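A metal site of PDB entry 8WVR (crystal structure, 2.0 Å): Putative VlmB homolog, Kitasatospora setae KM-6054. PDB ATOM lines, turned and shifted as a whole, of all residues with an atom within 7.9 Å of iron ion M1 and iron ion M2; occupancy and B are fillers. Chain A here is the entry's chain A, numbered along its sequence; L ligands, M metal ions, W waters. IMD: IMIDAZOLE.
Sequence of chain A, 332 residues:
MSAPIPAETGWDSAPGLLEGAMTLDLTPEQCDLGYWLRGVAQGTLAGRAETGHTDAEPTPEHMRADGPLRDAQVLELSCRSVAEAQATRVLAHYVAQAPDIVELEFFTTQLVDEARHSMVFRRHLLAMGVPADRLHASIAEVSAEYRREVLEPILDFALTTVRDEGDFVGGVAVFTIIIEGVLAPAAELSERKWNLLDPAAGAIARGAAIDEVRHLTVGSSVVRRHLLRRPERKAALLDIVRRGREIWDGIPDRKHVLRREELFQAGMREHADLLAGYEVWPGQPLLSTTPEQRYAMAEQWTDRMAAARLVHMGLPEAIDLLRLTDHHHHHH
NE2 of Gln 110 is in hydrogen-bond range of OE1 of Glu 180 (3.0 Å). The backbone NH (N) of Glu 180 sits at hydrogen-bond distance from the backbone carbonyl oxygen (O) of Phe 175 (2.8 Å). A ring nitrogen (ND1) of His 215 lies close to the side-chain amide nitrogen (NE2) of Gln 110 (3.5 Å). The side-chain carboxylate of Asp 113 is in hydrogen-bond range of a ring nitrogen (NE2) of His 215. OE2 of Glu 114 lies close to NE2 of Gln 110, at 3.2 Å. A ring nitrogen (NE2) of His 117 sits close to the backbone carbonyl oxygen (O) of Asp 113, 3.5 Å away. A ring nitrogen (NE2) of His 117 sits at hydrogen-bond distance from the side-chain carboxylate (OD2) of Asp 211, 2.8 Å away.
Of the 25 residues printed, 3 come within 4 Å of iron ion M1. The nearest printed residue that does not touch iron ion M1 is Glu 180 (4.4 Å).
Residues that only touch iron ion M2: Gln 110 (3.8 Å). Along chain A the residues within 4 Å of iron ion M2 span positions 110 to 215. The nearest printed residue that does not touch iron ion M2 is His 117 (4.6 Å).
Iron ion M1 is bound by water W1, OE2 of Glu 84, OE1 of Glu 114, ND1 of His 117 and N1 of the ligand. Iron ion M1 has five donor atoms within binding distance.
Iron ion M2 is bound by the side-chain carboxylate (OE2) of Glu 180, water W1, a ring nitrogen (ND1) of His 215, the side-chain carboxylate (OE1) of Glu 212 and the side-chain carboxylate (OE2) of Glu 114.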
ATOM      1  N   ARG A  80     -17.587 -28.960  21.560  1.00  0.00           N
ATOM      2  CA  ARG A  80     -16.886 -27.822  22.146  1.00  0.00           C
ATOM      3  C   ARG A  80     -17.330 -27.560  23.577  1.00  0.00           C
ATOM      4  O   ARG A  80     -16.511 -27.252  24.452  1.00  0.00           O
ATOM      5  CB  ARG A  80     -17.091 -26.577  21.289  1.00  0.00           C
ATOM      6  CG  ARG A  80     -16.323 -26.580  19.969  1.00  0.00           C
ATOM      7  CD  ARG A  80     -16.394 -25.229  19.302  1.00  0.00           C
ATOM      8  NE  ARG A  80     -15.746 -25.266  17.995  1.00  0.00           N
ATOM      9  CZ  ARG A  80     -14.437 -25.296  17.833  1.00  0.00           C
ATOM     10  NH1 ARG A  80     -13.605 -25.282  18.872  1.00  0.00           N
ATOM     11  NH2 ARG A  80     -13.928 -25.357  16.604  1.00  0.00           N
ATOM     12  N   ALA A  83     -15.686 -30.064  25.763  1.00  0.00           N
ATOM     13  CA  ALA A  83     -14.239 -29.838  25.816  1.00  0.00           C
ATOM     14  C   ALA A  83     -13.899 -28.677  26.740  1.00  0.00           C
ATOM     15  O   ALA A  83     -12.957 -28.764  27.537  1.00  0.00           O
ATOM     16  CB  ALA A  83     -13.710 -29.578  24.390  1.00  0.00           C
ATOM     17  N   GLU A  84     -14.652 -27.580  26.639  1.00  0.00           N
ATOM     18  CA  GLU A  84     -14.386 -26.400  27.440  1.00  0.00           C
ATOM     19  C   GLU A  84     -14.704 -26.642  28.912  1.00  0.00           C
ATOM     20  O   GLU A  84     -14.026 -26.084  29.788  1.00  0.00           O
ATOM     21  CB  GLU A  84     -15.175 -25.203  26.896  1.00  0.00           C
ATOM     22  CG  GLU A  84     -14.786 -24.772  25.469  1.00  0.00           C
ATOM     23  CD  GLU A  84     -13.358 -24.268  25.365  1.00  0.00           C
ATOM     24  OE1 GLU A  84     -12.411 -25.021  25.713  1.00  0.00           O
ATOM     25  OE2 GLU A  84     -13.170 -23.100  24.944  1.00  0.00           O
ATOM     26  N   ALA A  87     -11.842 -28.716  30.196  1.00  0.00           N
ATOM     27  CA  ALA A  87     -10.671 -27.861  30.287  1.00  0.00           C
ATOM     28  C   ALA A  87     -10.707 -26.994  31.536  1.00  0.00           C
ATOM     29  O   ALA A  87      -9.670 -26.741  32.163  1.00  0.00           O
ATOM     30  CB  ALA A  87     -10.561 -26.983  29.028  1.00  0.00           C
ATOM     31  N   LEU A  91      -7.800 -26.850  34.169  1.00  0.00           N
ATOM     32  CA  LEU A  91      -7.179 -25.578  34.507  1.00  0.00           C
ATOM     33  C   LEU A  91      -7.256 -25.265  36.006  1.00  0.00           C
ATOM     34  O   LEU A  91      -6.424 -24.521  36.525  1.00  0.00           O
ATOM     35  CB  LEU A  91      -7.849 -24.459  33.704  1.00  0.00           C
ATOM     36  CG  LEU A  91      -7.393 -24.454  32.232  1.00  0.00           C
ATOM     37  CD1 LEU A  91      -8.297 -23.530  31.432  1.00  0.00           C
ATOM     38  CD2 LEU A  91      -5.895 -24.066  32.059  1.00  0.00           C
ATOM     39  N   GLN A 110      -8.305 -17.331  32.891  1.00  0.00           N
ATOM     40  CA  GLN A 110      -8.473 -18.269  31.791  1.00  0.00           C
ATOM     41  C   GLN A 110      -9.450 -19.363  32.163  1.00  0.00           C
ATOM     42  O   GLN A 110     -10.267 -19.786  31.331  1.00  0.00           O
ATOM     43  CB  GLN A 110      -7.127 -18.870  31.360  1.00  0.00           C
ATOM     44  CG  GLN A 110      -7.347 -19.960  30.308  1.00  0.00           C
ATOM     45  CD  GLN A 110      -6.098 -20.379  29.543  1.00  0.00           C
ATOM     46  OE1 GLN A 110      -4.988 -19.931  29.840  1.00  0.00           O
ATOM     47  NE2 GLN A 110      -6.285 -21.243  28.542  1.00  0.00           N
ATOM     48  N   ASP A 113     -12.743 -17.926  31.614  1.00  0.00           N
ATOM     49  CA  ASP A 113     -12.957 -17.828  30.166  1.00  0.00           C
ATOM     50  C   ASP A 113     -13.434 -19.152  29.612  1.00  0.00           C
ATOM     51  O   ASP A 113     -14.414 -19.201  28.851  1.00  0.00           O
ATOM     52  CB  ASP A 113     -11.647 -17.407  29.451  1.00  0.00           C
ATOM     53  CG  ASP A 113     -11.326 -15.939  29.610  1.00  0.00           C
ATOM     54  OD1 ASP A 113     -12.228 -15.150  29.935  1.00  0.00           O
ATOM     55  OD2 ASP A 113     -10.143 -15.566  29.382  1.00  0.00           O
ATOM     56  N   GLU A 114     -12.771 -20.253  29.975  1.00  0.00           N
ATOM     57  CA  GLU A 114     -13.164 -21.534  29.395  1.00  0.00           C
ATOM     58  C   GLU A 114     -14.530 -21.976  29.894  1.00  0.00           C
ATOM     59  O   GLU A 114     -15.315 -22.567  29.142  1.00  0.00           O
ATOM     60  CB  GLU A 114     -12.121 -22.616  29.711  1.00  0.00           C
ATOM     61  CG  GLU A 114     -10.687 -22.308  29.332  1.00  0.00           C
ATOM     62  CD  GLU A 114     -10.452 -21.987  27.848  1.00  0.00           C
ATOM     63  OE1 GLU A 114     -11.347 -22.157  27.018  1.00  0.00           O
ATOM     64  OE2 GLU A 114      -9.326 -21.572  27.526  1.00  0.00           O
ATOM     65  N   ALA A 115     -14.830 -21.704  31.162  1.00  0.00           N
ATOM     66  CA  ALA A 115     -16.166 -22.004  31.653  1.00  0.00           C
ATOM     67  C   ALA A 115     -17.205 -21.196  30.893  1.00  0.00           C
ATOM     68  O   ALA A 115     -18.292 -21.705  30.579  1.00  0.00           O
ATOM     69  CB  ALA A 115     -16.261 -21.737  33.151  1.00  0.00           C
ATOM     70  N   ARG A 116     -16.891 -19.931  30.576  1.00  0.00           N
ATOM     71  CA  ARG A 116     -17.797 -19.115  29.762  1.00  0.00           C
ATOM     72  C   ARG A 116     -17.971 -19.706  28.362  1.00  0.00           C
ATOM     73  O   ARG A 116     -19.096 -19.767  27.851  1.00  0.00           O
ATOM     74  CB  ARG A 116     -17.265 -17.681  29.667  1.00  0.00           C
ATOM     75  CG  ARG A 116     -18.315 -16.691  29.136  1.00  0.00           C
ATOM     76  CD  ARG A 116     -17.726 -15.317  28.856  1.00  0.00           C
ATOM     77  NE  ARG A 116     -16.798 -15.325  27.719  1.00  0.00           N
ATOM     78  CZ  ARG A 116     -17.173 -15.464  26.460  1.00  0.00           C
ATOM     79  NH1 ARG A 116     -18.454 -15.588  26.117  1.00  0.00           N
ATOM     80  NH2 ARG A 116     -16.239 -15.466  25.497  1.00  0.00           N
ATOM     81  N   HIS A 117     -16.874 -20.137  27.731  1.00  0.00           N
ATOM     82  CA  HIS A 117     -16.979 -20.761  26.424  1.00  0.00           C
ATOM     83  C   HIS A 117     -17.899 -21.964  26.472  1.00  0.00           C
ATOM     84  O   HIS A 117     -18.777 -22.110  25.621  1.00  0.00           O
ATOM     85  CB  HIS A 117     -15.587 -21.168  25.929  1.00  0.00           C
ATOM     86  CG  HIS A 117     -14.671 -20.001  25.776  1.00  0.00           C
ATOM     87  ND1 HIS A 117     -13.326 -20.117  25.538  1.00  0.00           N
ATOM     88  CD2 HIS A 117     -14.930 -18.668  25.854  1.00  0.00           C
ATOM     89  CE1 HIS A 117     -12.790 -18.912  25.462  1.00  0.00           C
ATOM     90  NE2 HIS A 117     -13.739 -18.015  25.671  1.00  0.00           N
ATOM     91  N   SER A 118     -17.716 -22.820  27.485  1.00  0.00           N
ATOM     92  CA  SER A 118     -18.607 -23.962  27.628  1.00  0.00           C
ATOM     93  C   SER A 118     -20.051 -23.495  27.719  1.00  0.00           C
ATOM     94  O   SER A 118     -20.948 -24.112  27.136  1.00  0.00           O
ATOM     95  CB  SER A 118     -18.261 -24.774  28.877  1.00  0.00           C
ATOM     96  OG  SER A 118     -19.049 -25.948  28.947  1.00  0.00           O
ATOM     97  N   PHE A 121     -21.507 -21.992  24.366  1.00  0.00           N
ATOM     98  CA  PHE A 121     -21.728 -23.062  23.407  1.00  0.00           C
ATOM     99  C   PHE A 121     -22.973 -23.869  23.759  1.00  0.00           C
ATOM    100  O   PHE A 121     -23.784 -24.176  22.878  1.00  0.00           O
ATOM    101  CB  PHE A 121     -20.489 -23.985  23.332  1.00  0.00           C
ATOM    102  CG  PHE A 121     -19.284 -23.338  22.699  1.00  0.00           C
ATOM    103  CD1 PHE A 121     -19.436 -22.398  21.699  1.00  0.00           C
ATOM    104  CD2 PHE A 121     -18.008 -23.660  23.120  1.00  0.00           C
ATOM    105  CE1 PHE A 121     -18.327 -21.782  21.115  1.00  0.00           C
ATOM    106  CE2 PHE A 121     -16.895 -23.072  22.553  1.00  0.00           C
ATOM    107  CZ  PHE A 121     -17.051 -22.125  21.548  1.00  0.00           C
ATOM    108  N   PHE A 175      -0.736 -27.363  27.734  1.00  0.00           N
ATOM    109  CA  PHE A 175      -2.003 -26.711  27.428  1.00  0.00           C
ATOM    110  C   PHE A 175      -1.863 -25.750  26.252  1.00  0.00           C
ATOM    111  O   PHE A 175      -2.740 -25.674  25.387  1.00  0.00           O
ATOM    112  CB  PHE A 175      -2.548 -25.991  28.662  1.00  0.00           C
ATOM    113  CG  PHE A 175      -4.049 -25.897  28.681  1.00  0.00           C
ATOM    114  CD1 PHE A 175      -4.704 -24.891  27.981  1.00  0.00           C
ATOM    115  CD2 PHE A 175      -4.804 -26.830  29.385  1.00  0.00           C
ATOM    116  CE1 PHE A 175      -6.095 -24.808  27.980  1.00  0.00           C
ATOM    117  CE2 PHE A 175      -6.204 -26.770  29.384  1.00  0.00           C
ATOM    118  CZ  PHE A 175      -6.847 -25.733  28.673  1.00  0.00           C
ATOM    119  N   GLU A 180      -4.342 -25.991  23.057  1.00  0.00           N
ATOM    120  CA  GLU A 180      -4.921 -24.802  22.426  1.00  0.00           C
ATOM    121  C   GLU A 180      -4.176 -24.444  21.146  1.00  0.00           C
ATOM    122  O   GLU A 180      -4.790 -24.044  20.154  1.00  0.00           O
ATOM    123  CB  GLU A 180      -4.922 -23.639  23.404  1.00  0.00           C
ATOM    124  CG  GLU A 180      -5.888 -23.888  24.581  1.00  0.00           C
ATOM    125  CD  GLU A 180      -6.323 -22.628  25.284  1.00  0.00           C
ATOM    126  OE1 GLU A 180      -5.442 -21.824  25.673  1.00  0.00           O
ATOM    127  OE2 GLU A 180      -7.553 -22.470  25.450  1.00  0.00           O
ATOM    128  N   ALA A 184      -6.899 -24.133  18.324  1.00  0.00           N
ATOM    129  CA  ALA A 184      -7.393 -22.784  18.038  1.00  0.00           C
ATOM    130  C   ALA A 184      -7.597 -22.506  16.541  1.00  0.00           C
ATOM    131  O   ALA A 184      -8.546 -21.774  16.222  1.00  0.00           O
ATOM    132  CB  ALA A 184      -6.461 -21.753  18.669  1.00  0.00           C
ATOM    133  N   ALA A 187     -10.935 -23.234  15.580  1.00  0.00           N
ATOM    134  CA  ALA A 187     -11.867 -22.252  16.126  1.00  0.00           C
ATOM    135  C   ALA A 187     -11.940 -21.021  15.226  1.00  0.00           C
ATOM    136  O   ALA A 187     -13.035 -20.514  14.940  1.00  0.00           O
ATOM    137  CB  ALA A 187     -11.475 -21.862  17.547  1.00  0.00           C
ATOM    138  N   ALA A 208     -14.968 -15.675  21.946  1.00  0.00           N
ATOM    139  CA  ALA A 208     -14.026 -16.697  22.416  1.00  0.00           C
ATOM    140  C   ALA A 208     -12.659 -16.561  21.750  1.00  0.00           C
ATOM    141  O   ALA A 208     -11.619 -16.794  22.386  1.00  0.00           O
ATOM    142  CB  ALA A 208     -14.622 -18.094  22.192  1.00  0.00           C
ATOM    143  N   ALA A 209     -12.641 -16.184  20.462  1.00  0.00           N
ATOM    144  CA  ALA A 209     -11.367 -16.034  19.753  1.00  0.00           C
ATOM    145  C   ALA A 209     -10.569 -14.880  20.342  1.00  0.00           C
ATOM    146  O   ALA A 209      -9.345 -14.978  20.489  1.00  0.00           O
ATOM    147  CB  ALA A 209     -11.597 -15.823  18.255  1.00  0.00           C
ATOM    148  N   ASP A 211     -10.707 -13.923  23.485  1.00  0.00           N
ATOM    149  CA  ASP A 211     -10.148 -14.557  24.679  1.00  0.00           C
ATOM    150  C   ASP A 211      -8.933 -15.402  24.317  1.00  0.00           C
ATOM    151  O   ASP A 211      -7.903 -15.344  24.992  1.00  0.00           O
ATOM    152  CB  ASP A 211     -11.203 -15.445  25.365  1.00  0.00           C
ATOM    153  CG  ASP A 211     -12.410 -14.672  25.883  1.00  0.00           C
ATOM    154  OD1 ASP A 211     -12.282 -13.481  26.246  1.00  0.00           O
ATOM    155  OD2 ASP A 211     -13.492 -15.285  25.948  1.00  0.00           O
ATOM    156  N   GLU A 212      -9.039 -16.194  23.255  1.00  0.00           N
ATOM    157  CA  GLU A 212      -8.001 -17.161  22.926  1.00  0.00           C
ATOM    158  C   GLU A 212      -6.707 -16.488  22.504  1.00  0.00           C
ATOM    159  O   GLU A 212      -5.617 -17.010  22.761  1.00  0.00           O
ATOM    160  CB  GLU A 212      -8.496 -18.123  21.840  1.00  0.00           C
ATOM    161  CG  GLU A 212      -7.580 -19.311  21.545  1.00  0.00           C
ATOM    162  CD  GLU A 212      -7.582 -20.371  22.648  1.00  0.00           C
ATOM    163  OE1 GLU A 212      -7.757 -20.012  23.816  1.00  0.00           O
ATOM    164  OE2 GLU A 212      -7.370 -21.558  22.357  1.00  0.00           O
ATOM    165  N   VAL A 213      -6.797 -15.306  21.874  1.00  0.00           N
ATOM    166  CA  VAL A 213      -5.584 -14.540  21.589  1.00  0.00           C
ATOM    167  C   VAL A 213      -4.796 -14.350  22.878  1.00  0.00           C
ATOM    168  O   VAL A 213      -3.570 -14.546  22.913  1.00  0.00           O
ATOM    169  CB  VAL A 213      -5.935 -13.193  20.938  1.00  0.00           C
ATOM    170  CG1 VAL A 213      -4.711 -12.285  20.904  1.00  0.00           C
ATOM    171  CG2 VAL A 213      -6.496 -13.388  19.533  1.00  0.00           C
ATOM    172  N   ARG A 214      -5.503 -13.983  23.946  1.00  0.00           N
ATOM    173  CA  ARG A 214      -4.878 -13.783  25.248  1.00  0.00           C
ATOM    174  C   ARG A 214      -4.363 -15.104  25.823  1.00  0.00           C
ATOM    175  O   ARG A 214      -3.238 -15.164  26.320  1.00  0.00           O
ATOM    176  CB  ARG A 214      -5.885 -13.119  26.197  1.00  0.00           C
ATOM    177  CG  ARG A 214      -5.395 -12.907  27.646  1.00  0.00           C
ATOM    178  CD  ARG A 214      -6.437 -12.140  28.497  1.00  0.00           C
ATOM    179  NE  ARG A 214      -7.743 -12.804  28.561  1.00  0.00           N
ATOM    180  CZ  ARG A 214      -8.795 -12.506  27.799  1.00  0.00           C
ATOM    181  NH1 ARG A 214      -8.741 -11.541  26.875  1.00  0.00           N
ATOM    182  NH2 ARG A 214      -9.929 -13.172  27.972  1.00  0.00           N
ATOM    183  N   HIS A 215      -5.170 -16.172  25.784  1.00  0.00           N
ATOM    184  CA  HIS A 215      -4.693 -17.455  26.313  1.00  0.00           C
ATOM    185  C   HIS A 215      -3.404 -17.883  25.624  1.00  0.00           C
ATOM    186  O   HIS A 215      -2.438 -18.294  26.284  1.00  0.00           O
ATOM    187  CB  HIS A 215      -5.755 -18.563  26.157  1.00  0.00           C
ATOM    188  CG  HIS A 215      -7.068 -18.261  26.814  1.00  0.00           C
ATOM    189  ND1 HIS A 215      -8.192 -19.057  26.644  1.00  0.00           N
ATOM    190  CD2 HIS A 215      -7.444 -17.257  27.647  1.00  0.00           C
ATOM    191  CE1 HIS A 215      -9.197 -18.540  27.325  1.00  0.00           C
ATOM    192  NE2 HIS A 215      -8.766 -17.453  27.949  1.00  0.00           N
ATOM    193  N   LEU A 216      -3.380 -17.791  24.292  1.00  0.00           N
ATOM    194  CA  LEU A 216      -2.246 -18.293  23.516  1.00  0.00           C
ATOM    195  C   LEU A 216      -0.996 -17.442  23.743  1.00  0.00           C
ATOM    196  O   LEU A 216       0.095 -17.984  23.942  1.00  0.00           O
ATOM    197  CB  LEU A 216      -2.620 -18.322  22.033  1.00  0.00           C
ATOM    198  CG  LEU A 216      -3.596 -19.435  21.660  1.00  0.00           C
ATOM    199  CD1 LEU A 216      -4.080 -19.252  20.212  1.00  0.00           C
ATOM    200  CD2 LEU A 216      -2.939 -20.799  21.857  1.00  0.00           C
HETATM  201  N1  IMD L   1     -12.265 -21.373  22.784  1.00  0.00           N
HETATM  202  C2  IMD L   1     -13.217 -21.890  21.965  1.00  0.00           C
HETATM  203  N3  IMD L   1     -13.167 -21.223  20.816  1.00  0.00           N
HETATM  204  C4  IMD L   1     -12.188 -20.278  20.898  1.00  0.00           C
HETATM  205  C5  IMD L   1     -11.632 -20.382  22.130  1.00  0.00           C
HETATM  206 FE    FE M   1     -11.876 -21.645  24.991  1.00  0.00          FE
HETATM  207 FE    FE M   2      -8.588 -20.848  25.588  1.00  0.00          FE
HETATM  208  O   HOH W   1     -10.430 -20.515  24.909  1.00  0.00           O
